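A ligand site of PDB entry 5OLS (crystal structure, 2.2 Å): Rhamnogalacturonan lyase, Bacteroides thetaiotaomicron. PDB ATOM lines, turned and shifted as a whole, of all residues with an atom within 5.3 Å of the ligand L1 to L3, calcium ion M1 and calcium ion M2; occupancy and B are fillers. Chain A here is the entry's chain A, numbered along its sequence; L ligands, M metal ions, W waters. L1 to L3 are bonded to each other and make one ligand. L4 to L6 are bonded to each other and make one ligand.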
ATOM      1  N   LYS A 189     -33.848 -27.032 -40.956  1.00  0.00           N
ATOM      2  CA  LYS A 189     -34.224 -26.986 -39.528  1.00  0.00           C
ATOM      3  C   LYS A 189     -33.994 -25.589 -38.939  1.00  0.00           C
ATOM      4  O   LYS A 189     -34.815 -25.093 -38.170  1.00  0.00           O
ATOM      5  CB  LYS A 189     -33.435 -28.037 -38.708  1.00  0.00           C
ATOM      6  CG  LYS A 189     -33.804 -28.134 -37.220  1.00  0.00           C
ATOM      7  CD  LYS A 189     -35.123 -28.867 -37.001  1.00  0.00           C
ATOM      8  CE  LYS A 189     -35.756 -28.573 -35.629  1.00  0.00           C
ATOM      9  NZ  LYS A 189     -35.417 -29.540 -34.555  1.00  0.00           N
ATOM     10  N   GLY A 191     -31.630 -24.947 -36.819  1.00  0.00           N
ATOM     11  CA  GLY A 191     -31.332 -25.210 -35.415  1.00  0.00           C
ATOM     12  C   GLY A 191     -30.054 -24.587 -34.851  1.00  0.00           C
ATOM     13  O   GLY A 191     -29.762 -24.757 -33.657  1.00  0.00           O
ATOM     14  N   ASN A 192     -29.289 -23.901 -35.690  1.00  0.00           N
ATOM     15  CA  ASN A 192     -28.015 -23.289 -35.301  1.00  0.00           C
ATOM     16  C   ASN A 192     -28.021 -21.755 -35.356  1.00  0.00           C
ATOM     17  O   ASN A 192     -27.033 -21.121 -34.956  1.00  0.00           O
ATOM     18  CB  ASN A 192     -26.906 -23.844 -36.195  1.00  0.00           C
ATOM     19  CG  ASN A 192     -26.620 -25.318 -35.938  1.00  0.00           C
ATOM     20  OD1 ASN A 192     -26.997 -25.877 -34.924  1.00  0.00           O
ATOM     21  ND2 ASN A 192     -25.919 -25.952 -36.874  1.00  0.00           N
ATOM     22  N   ASP A 194     -29.058 -18.531 -33.963  1.00  0.00           N
ATOM     23  CA  ASP A 194     -29.467 -17.657 -32.873  1.00  0.00           C
ATOM     24  C   ASP A 194     -29.277 -16.181 -33.200  1.00  0.00           C
ATOM     25  O   ASP A 194     -28.469 -15.802 -34.077  1.00  0.00           O
ATOM     26  CB  ASP A 194     -28.654 -17.947 -31.591  1.00  0.00           C
ATOM     27  CG  ASP A 194     -28.916 -19.334 -30.999  1.00  0.00           C
ATOM     28  OD1 ASP A 194     -29.956 -19.975 -31.286  1.00  0.00           O
ATOM     29  OD2 ASP A 194     -28.063 -19.808 -30.209  1.00  0.00           O
ATOM     30  N   HIS A 199     -20.880 -18.051 -25.816  1.00  0.00           N
ATOM     31  CA  HIS A 199     -20.339 -19.421 -25.719  1.00  0.00           C
ATOM     32  C   HIS A 199     -18.825 -19.396 -25.468  1.00  0.00           C
ATOM     33  O   HIS A 199     -18.031 -20.019 -26.199  1.00  0.00           O
ATOM     34  CB  HIS A 199     -20.663 -20.216 -26.980  1.00  0.00           C
ATOM     35  CG  HIS A 199     -22.084 -20.068 -27.430  1.00  0.00           C
ATOM     36  ND1 HIS A 199     -23.141 -20.498 -26.674  1.00  0.00           N
ATOM     37  CD2 HIS A 199     -22.602 -19.504 -28.536  1.00  0.00           C
ATOM     38  CE1 HIS A 199     -24.265 -20.222 -27.304  1.00  0.00           C
ATOM     39  NE2 HIS A 199     -23.969 -19.619 -28.442  1.00  0.00           N
ATOM     40  N   ASP A 225     -33.679 -20.499 -34.467  1.00  0.00           N
ATOM     41  CA  ASP A 225     -33.435 -21.261 -33.237  1.00  0.00           C
ATOM     42  C   ASP A 225     -33.841 -20.464 -31.964  1.00  0.00           C
ATOM     43  O   ASP A 225     -35.024 -20.473 -31.561  1.00  0.00           O
ATOM     44  CB  ASP A 225     -32.000 -21.795 -33.198  1.00  0.00           C
ATOM     45  CG  ASP A 225     -31.789 -22.873 -32.139  1.00  0.00           C
ATOM     46  OD1 ASP A 225     -32.571 -23.857 -32.119  1.00  0.00           O
ATOM     47  OD2 ASP A 225     -30.794 -22.767 -31.352  1.00  0.00           O
ATOM     48  N   ASP A 226     -32.895 -19.763 -31.342  1.00  0.00           N
ATOM     49  CA  ASP A 226     -33.169 -19.003 -30.136  1.00  0.00           C
ATOM     50  C   ASP A 226     -32.918 -17.535 -30.398  1.00  0.00           C
ATOM     51  O   ASP A 226     -32.283 -17.151 -31.401  1.00  0.00           O
ATOM     52  CB  ASP A 226     -32.297 -19.504 -28.995  1.00  0.00           C
ATOM     53  CG  ASP A 226     -32.496 -20.984 -28.718  1.00  0.00           C
ATOM     54  OD1 ASP A 226     -33.645 -21.484 -28.726  1.00  0.00           O
ATOM     55  OD2 ASP A 226     -31.498 -21.657 -28.444  1.00  0.00           O
ATOM     56  N   ASP A 229     -28.758 -17.209 -26.300  1.00  0.00           N
ATOM     57  CA  ASP A 229     -28.308 -18.551 -25.929  1.00  0.00           C
ATOM     58  C   ASP A 229     -26.918 -18.464 -25.286  1.00  0.00           C
ATOM     59  O   ASP A 229     -25.977 -17.943 -25.909  1.00  0.00           O
ATOM     60  CB  ASP A 229     -28.282 -19.411 -27.196  1.00  0.00           C
ATOM     61  CG  ASP A 229     -27.864 -20.861 -26.955  1.00  0.00           C
ATOM     62  OD1 ASP A 229     -27.416 -21.204 -25.838  1.00  0.00           O
ATOM     63  OD2 ASP A 229     -27.984 -21.654 -27.932  1.00  0.00           O
ATOM     64  N   ILE A 231     -25.302 -21.378 -23.874  1.00  0.00           N
ATOM     65  CA  ILE A 231     -24.842 -22.735 -23.673  1.00  0.00           C
ATOM     66  C   ILE A 231     -23.336 -22.748 -23.860  1.00  0.00           C
ATOM     67  O   ILE A 231     -22.800 -21.936 -24.613  1.00  0.00           O
ATOM     68  CB  ILE A 231     -25.541 -23.738 -24.633  1.00  0.00           C
ATOM     69  CG1 ILE A 231     -25.585 -25.132 -23.993  1.00  0.00           C
ATOM     70  CG2 ILE A 231     -24.863 -23.761 -26.012  1.00  0.00           C
ATOM     71  CD1 ILE A 231     -26.191 -26.214 -24.871  1.00  0.00           C
ATOM     72  N   ASP A 259     -35.316 -24.438 -31.641  1.00  0.00           N
ATOM     73  CA  ASP A 259     -35.716 -24.679 -30.242  1.00  0.00           C
ATOM     74  C   ASP A 259     -36.658 -23.665 -29.637  1.00  0.00           C
ATOM     75  O   ASP A 259     -37.322 -23.953 -28.635  1.00  0.00           O
ATOM     76  CB  ASP A 259     -34.481 -24.794 -29.347  1.00  0.00           C
ATOM     77  CG  ASP A 259     -33.540 -25.886 -29.805  1.00  0.00           C
ATOM     78  OD1 ASP A 259     -33.977 -26.765 -30.551  1.00  0.00           O
ATOM     79  OD2 ASP A 259     -32.357 -25.847 -29.447  1.00  0.00           O
ATOM     80  N   GLY A 267     -26.351 -23.941 -19.516  1.00  0.00           N
ATOM     81  CA  GLY A 267     -26.356 -25.299 -20.019  1.00  0.00           C
ATOM     82  C   GLY A 267     -25.025 -25.727 -20.585  1.00  0.00           C
ATOM     83  O   GLY A 267     -24.259 -24.903 -21.091  1.00  0.00           O
ATOM     84  N   GLY A 269     -25.288 -28.986 -22.272  1.00  0.00           N
ATOM     85  CA  GLY A 269     -25.827 -30.113 -23.006  1.00  0.00           C
ATOM     86  C   GLY A 269     -26.194 -31.287 -22.118  1.00  0.00           C
ATOM     87  O   GLY A 269     -25.724 -31.420 -20.983  1.00  0.00           O
ATOM     88  N   MET A 270     -27.022 -32.147 -22.684  1.00  0.00           N
ATOM     89  CA  MET A 270     -27.418 -33.393 -22.060  1.00  0.00           C
ATOM     90  C   MET A 270     -26.983 -34.528 -22.992  1.00  0.00           C
ATOM     91  O   MET A 270     -27.781 -35.386 -23.352  1.00  0.00           O
ATOM     92  CB  MET A 270     -28.931 -33.406 -21.848  1.00  0.00           C
ATOM     93  CG  MET A 270     -29.431 -32.305 -20.929  1.00  0.00           C
ATOM     94  SD  MET A 270     -29.072 -32.679 -19.213  1.00  0.00           S
ATOM     95  CE  MET A 270     -30.425 -33.790 -18.852  1.00  0.00           C
ATOM     96  N   ARG A 296     -41.334 -19.944 -29.605  1.00  0.00           N
ATOM     97  CA  ARG A 296     -42.036 -21.182 -29.907  1.00  0.00           C
ATOM     98  C   ARG A 296     -42.317 -22.012 -28.649  1.00  0.00           C
ATOM     99  O   ARG A 296     -43.439 -22.494 -28.477  1.00  0.00           O
ATOM    100  CB  ARG A 296     -41.314 -22.046 -30.949  1.00  0.00           C
ATOM    101  CG  ARG A 296     -42.175 -23.155 -31.526  1.00  0.00           C
ATOM    102  CD  ARG A 296     -41.541 -23.822 -32.747  1.00  0.00           C
ATOM    103  NE  ARG A 296     -40.438 -24.721 -32.400  1.00  0.00           N
ATOM    104  CZ  ARG A 296     -40.576 -25.935 -31.854  1.00  0.00           C
ATOM    105  NH1 ARG A 296     -39.492 -26.651 -31.576  1.00  0.00           N
ATOM    106  NH2 ARG A 296     -41.782 -26.441 -31.576  1.00  0.00           N
ATOM    107  N   LEU A 297     -41.326 -22.159 -27.775  1.00  0.00           N
ATOM    108  CA  LEU A 297     -41.404 -23.136 -26.680  1.00  0.00           C
ATOM    109  C   LEU A 297     -41.194 -22.563 -25.292  1.00  0.00           C
ATOM    110  O   LEU A 297     -41.938 -22.910 -24.377  1.00  0.00           O
ATOM    111  CB  LEU A 297     -40.411 -24.290 -26.906  1.00  0.00           C
ATOM    112  CG  LEU A 297     -40.836 -25.357 -27.923  1.00  0.00           C
ATOM    113  CD1 LEU A 297     -39.737 -26.394 -28.157  1.00  0.00           C
ATOM    114  CD2 LEU A 297     -42.127 -26.058 -27.489  1.00  0.00           C
ATOM    115  N   ARG A 298     -40.181 -21.726 -25.113  1.00  0.00           N
ATOM    116  CA  ARG A 298     -39.821 -21.256 -23.781  1.00  0.00           C
ATOM    117  C   ARG A 298     -39.326 -19.789 -23.795  1.00  0.00           C
ATOM    118  O   ARG A 298     -38.831 -19.282 -24.814  1.00  0.00           O
ATOM    119  CB  ARG A 298     -38.771 -22.175 -23.146  1.00  0.00           C
ATOM    120  CG  ARG A 298     -38.973 -23.691 -23.293  1.00  0.00           C
ATOM    121  CD  ARG A 298     -37.781 -24.436 -22.687  1.00  0.00           C
ATOM    122  NE  ARG A 298     -37.945 -25.881 -22.549  1.00  0.00           N
ATOM    123  CZ  ARG A 298     -37.701 -26.795 -23.499  1.00  0.00           C
ATOM    124  NH1 ARG A 298     -37.328 -26.456 -24.730  1.00  0.00           N
ATOM    125  NH2 ARG A 298     -37.860 -28.079 -23.222  1.00  0.00           N
ATOM    126  N   TYR A 301     -35.074 -19.543 -19.537  1.00  0.00           N
ATOM    127  CA  TYR A 301     -34.771 -20.974 -19.431  1.00  0.00           C
ATOM    128  C   TYR A 301     -33.335 -21.235 -18.971  1.00  0.00           C
ATOM    129  O   TYR A 301     -32.386 -20.710 -19.544  1.00  0.00           O
ATOM    130  CB  TYR A 301     -34.997 -21.601 -20.805  1.00  0.00           C
ATOM    131  CG  TYR A 301     -34.854 -23.111 -20.938  1.00  0.00           C
ATOM    132  CD1 TYR A 301     -35.225 -23.996 -19.927  1.00  0.00           C
ATOM    133  CD2 TYR A 301     -34.387 -23.663 -22.139  1.00  0.00           C
ATOM    134  CE1 TYR A 301     -35.114 -25.385 -20.082  1.00  0.00           C
ATOM    135  CE2 TYR A 301     -34.284 -25.042 -22.309  1.00  0.00           C
ATOM    136  CZ  TYR A 301     -34.641 -25.905 -21.279  1.00  0.00           C
ATOM    137  OH  TYR A 301     -34.523 -27.276 -21.465  1.00  0.00           O
ATOM    138  N   ASN A 303     -31.869 -24.158 -18.994  1.00  0.00           N
ATOM    139  CA  ASN A 303     -31.308 -24.899 -20.106  1.00  0.00           C
ATOM    140  C   ASN A 303     -30.301 -25.952 -19.612  1.00  0.00           C
ATOM    141  O   ASN A 303     -29.233 -26.068 -20.164  1.00  0.00           O
ATOM    142  CB  ASN A 303     -30.652 -23.921 -21.104  1.00  0.00           C
ATOM    143  CG  ASN A 303     -30.421 -24.530 -22.477  1.00  0.00           C
ATOM    144  OD1 ASN A 303     -31.290 -25.209 -23.008  1.00  0.00           O
ATOM    145  ND2 ASN A 303     -29.247 -24.274 -23.055  1.00  0.00           N
ATOM    146  N   HIS A 304     -30.677 -26.683 -18.565  1.00  0.00           N
ATOM    147  CA  HIS A 304     -29.838 -27.762 -18.011  1.00  0.00           C
ATOM    148  C   HIS A 304     -28.492 -27.262 -17.445  1.00  0.00           C
ATOM    149  O   HIS A 304     -27.464 -27.927 -17.572  1.00  0.00           O
ATOM    150  CB  HIS A 304     -29.639 -28.884 -19.057  1.00  0.00           C
ATOM    151  CG  HIS A 304     -30.868 -29.208 -19.847  1.00  0.00           C
ATOM    152  ND1 HIS A 304     -31.822 -30.100 -19.402  1.00  0.00           N
ATOM    153  CD2 HIS A 304     -31.315 -28.729 -21.033  1.00  0.00           C
ATOM    154  CE1 HIS A 304     -32.801 -30.169 -20.291  1.00  0.00           C
ATOM    155  NE2 HIS A 304     -32.514 -29.342 -21.294  1.00  0.00           N
HETATM  156  C1  LIG L   1     -36.706 -29.710 -27.574  1.00  0.00           C
HETATM  157  C2  LIG L   1     -35.606 -29.611 -28.617  1.00  0.00           C
HETATM  158  C3  LIG L   1     -34.510 -30.608 -28.225  1.00  0.00           C
HETATM  159  C4  LIG L   1     -33.967 -30.280 -26.834  1.00  0.00           C
HETATM  160  C5  LIG L   1     -35.119 -30.083 -25.808  1.00  0.00           C
HETATM  161  C6  LIG L   1     -34.620 -29.549 -24.482  1.00  0.00           C
HETATM  162  O1  LIG L   1     -37.821 -28.934 -28.006  1.00  0.00           O
HETATM  163  O2  LIG L   1     -36.089 -29.830 -29.945  1.00  0.00           O
HETATM  164  O3  LIG L   1     -33.457 -30.541 -29.212  1.00  0.00           O
HETATM  165  O4  LIG L   1     -33.160 -29.083 -27.070  1.00  0.00           O
HETATM  166  O5  LIG L   1     -36.156 -29.222 -26.331  1.00  0.00           O
HETATM  167  O6  LIG L   1     -34.712 -28.323 -24.273  1.00  0.00           O
HETATM  168  O7  LIG L   1     -34.141 -30.324 -23.621  1.00  0.00           O
HETATM  169  C1  LG2 L   2     -31.935 -28.889 -26.297  1.00  0.00           C
HETATM  170  C2  LG2 L   2     -31.034 -27.725 -26.721  1.00  0.00           C
HETATM  171  C3  LG2 L   2     -30.547 -27.224 -25.358  1.00  0.00           C
HETATM  172  C4  LG2 L   2     -29.737 -28.315 -24.666  1.00  0.00           C
HETATM  173  C5  LG2 L   2     -30.585 -29.598 -24.515  1.00  0.00           C
HETATM  174  C6  LG2 L   2     -29.806 -30.767 -23.961  1.00  0.00           C
HETATM  175  O1  LG2 L   2     -29.947 -28.206 -27.582  1.00  0.00           O
HETATM  176  O2  LG2 L   2     -29.811 -26.013 -25.495  1.00  0.00           O
HETATM  177  O3  LG2 L   2     -29.254 -27.826 -23.399  1.00  0.00           O
HETATM  178  O4  LG2 L   2     -31.178 -29.987 -25.763  1.00  0.00           O
HETATM  179  O1  LG3 L   3     -27.271 -24.199 -28.250  1.00  0.00           O
HETATM  180  C1  LG3 L   3     -28.339 -24.769 -28.788  1.00  0.00           C
HETATM  181  O2  LG3 L   3     -29.256 -24.046 -29.190  1.00  0.00           O
HETATM  182  C2  LG3 L   3     -28.416 -26.092 -28.917  1.00  0.00           C
HETATM  183  O3  LG3 L   3     -29.623 -26.661 -29.498  1.00  0.00           O
HETATM  184  C3  LG3 L   3     -27.412 -26.922 -28.539  1.00  0.00           C
HETATM  185  C4  LG3 L   3     -27.449 -28.411 -28.861  1.00  0.00           C
HETATM  186  O4  LG3 L   3     -26.312 -28.750 -29.671  1.00  0.00           O
HETATM  187  C5  LG3 L   3     -28.728 -28.813 -29.595  1.00  0.00           C
HETATM  188  O5  LG3 L   3     -28.913 -30.231 -29.442  1.00  0.00           O
HETATM  189  C6  LG3 L   3     -29.898 -27.996 -29.048  1.00  0.00           C
HETATM  190  C1  LG4 L   4     -24.129 -26.252 -30.392  1.00  0.00           C
HETATM  191  C2  LG4 L   4     -23.180 -26.429 -31.583  1.00  0.00           C
HETATM  192  C3  LG4 L   4     -23.486 -25.355 -32.606  1.00  0.00           C
HETATM  193  C4  LG4 L   4     -23.520 -23.956 -31.992  1.00  0.00           C
HETATM  194  C5  LG4 L   4     -24.378 -23.884 -30.734  1.00  0.00           C
HETATM  195  C6  LG4 L   4     -24.211 -22.553 -30.010  1.00  0.00           C
HETATM  196  O1  LG4 L   4     -25.472 -26.481 -30.826  1.00  0.00           O
HETATM  197  O2  LG4 L   4     -21.826 -26.282 -31.131  1.00  0.00           O
HETATM  198  O3  LG4 L   4     -22.516 -25.387 -33.652  1.00  0.00           O
HETATM  199  O4  LG4 L   4     -24.039 -23.049 -32.970  1.00  0.00           O
HETATM  200  O5  LG4 L   4     -23.998 -24.932 -29.838  1.00  0.00           O
HETATM  201  C1  LG5 L   5     -20.918 -27.375 -31.429  1.00  0.00           C
HETATM  202  C2  LG5 L   5     -19.804 -27.347 -30.390  1.00  0.00           C
HETATM  203  C3  LG5 L   5     -18.941 -26.099 -30.545  1.00  0.00           C
HETATM  204  C4  LG5 L   5     -18.412 -25.938 -31.960  1.00  0.00           C
HETATM  205  C5  LG5 L   5     -19.596 -26.084 -32.933  1.00  0.00           C
HETATM  206  C6  LG5 L   5     -19.269 -25.933 -34.390  1.00  0.00           C
HETATM  207  O1  LG5 L   5     -20.382 -27.370 -29.082  1.00  0.00           O
HETATM  208  O2  LG5 L   5     -17.849 -26.201 -29.618  1.00  0.00           O
HETATM  209  O3  LG5 L   5     -17.424 -26.952 -32.107  1.00  0.00           O
HETATM  210  O4  LG5 L   5     -20.281 -27.325 -32.712  1.00  0.00           O
HETATM  211  O5  LG5 L   5     -19.444 -26.921 -35.137  1.00  0.00           O
HETATM  212  O6  LG5 L   5     -18.883 -24.823 -34.808  1.00  0.00           O
HETATM  213  C1  LG6 L   6     -16.085 -26.601 -32.375  1.00  0.00           C
HETATM  214  C2  LG6 L   6     -15.077 -27.474 -31.714  1.00  0.00           C
HETATM  215  C3  LG6 L   6     -14.927 -28.703 -32.580  1.00  0.00           C
HETATM  216  C4  LG6 L   6     -14.700 -28.311 -34.038  1.00  0.00           C
HETATM  217  C5  LG6 L   6     -15.521 -27.090 -34.537  1.00  0.00           C
HETATM  218  C6  LG6 L   6     -14.901 -26.555 -35.826  1.00  0.00           C
HETATM  219  O1  LG6 L   6     -13.822 -26.769 -31.592  1.00  0.00           O
HETATM  220  O2  LG6 L   6     -13.849 -29.477 -32.050  1.00  0.00           O
HETATM  221  O3  LG6 L   6     -15.073 -29.448 -34.828  1.00  0.00           O
HETATM  222  O4  LG6 L   6     -15.678 -26.016 -33.570  1.00  0.00           O
HETATM  223 CA    CA M   1     -29.473 -21.792 -29.908  1.00  0.00          CA
HETATM  224 CA    CA M   2     -30.362 -25.482 -31.421  1.00  0.00          CA
HETATM  225  O   HOH W   1     -27.894 -22.710 -31.350  1.00  0.00           O
HETATM  226  O   HOH W   2     -30.669 -27.565 -32.591  1.00  0.00           O
HETATM  227  O   HOH W   3     -31.651 -24.091 -27.722  1.00  0.00           O
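NE2 of His 304 is in hydrogen-bond range of O7 of LIG L1, at 3.0 Å. The side-chain hydroxyl of Tyr 301 sits at hydrogen-bond distance from an oxygen (O6) of LIG L1, at 3.0 Å. The side-chain amide oxygen (OD1) of Asn 303 sits at hydrogen-bond distance from an oxygen (O2) of LG2 L2. The guanidinium group (NH1) of Arg 298 lies within salt-bridge range of an oxygen (O6) of LIG L1 (3.2 Å).
An oxygen (O4) of LG3 L3 sits at hydrogen-bond distance from an oxygen (O1) of LG4 L4 (2.7 Å).
The side-chain sulfur (SD) of Met 270 sits close to a ring nitrogen (ND1) of His 304 (3.8 Å). OH of Tyr 301 lies within hydrogen-bond range of NE2 of His 304 (2.9 Å). The side-chain carboxylate (OD1) of Asp 229 is in hydrogen-bond range of the backbone NH (N) of Ile 231 (2.9 Å). ND1 of His 199 sits at hydrogen-bond distance from O of Ile 231 (2.5 Å).
Ile 231 touches the ligand L1 to L3. N of Met 270 touches C6 of LG2 L2, 3.4 Å away. Leu 297 touches the ligand L1 to L3. Hydrophobic or aromatic side chains that line the ligand L1 to L3: Ile 231, Met 270, Leu 297, Tyr 301 and His 304. Along chain A the residues within 4 Å of the ligand L1 to L3 span positions 225 to 304. The nearest printed residue that does not touch the ligand L1 to L3 is Gly 269 (4.1 Å).
Four residues have an atom within 4 Å of calcium ion M1: Asp 194, Asp 225, Asp 226 and Asp 229.
Three residues have an atom within 4 Å of calcium ion M2: Gly 191, Asp 225 and Asp 259.
OD2 of Asp 225 is bound to calcium ion M1. Water W1 binds calcium ion M1 (2.3 Å). OD1 of Asp 194 is bound to calcium ion M1. O2 of LG3 L3 is bound to calcium ion M1 (2.4 Å). OD2 of Asp 194 binds calcium ion M1, at 2.5 Å. OD2 of Asp 229 binds calcium ion M1 (2.5 Å). The side-chain carboxylate (OD2) of Asp 226 binds calcium ion M1 (2.5 Å).
Calcium ion M2 is bound by O3 of LG3 L3, 2.4 Å away. Water W2 is bound to calcium ion M2 (2.4 Å). The backbone carbonyl oxygen (O) of Gly 191 binds calcium ion M2 (2.4 Å). OD2 of Asp 225 is bound to calcium ion M2, 2.8 Å away. The side-chain carboxylate (OD1) of Asp 225 binds calcium ion M2, at 2.8 Å. Calcium ion M2 is bound by OD2 of Asp 259 (2.8 Å). Calcium ion M2 is bound by O2 of LG3 L3 (2.9 Å). Calcium ion M2 has seven donor atoms within binding distance.
Water W3 bridges OD1 of Asp 226 and O2 of LG2 L2.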
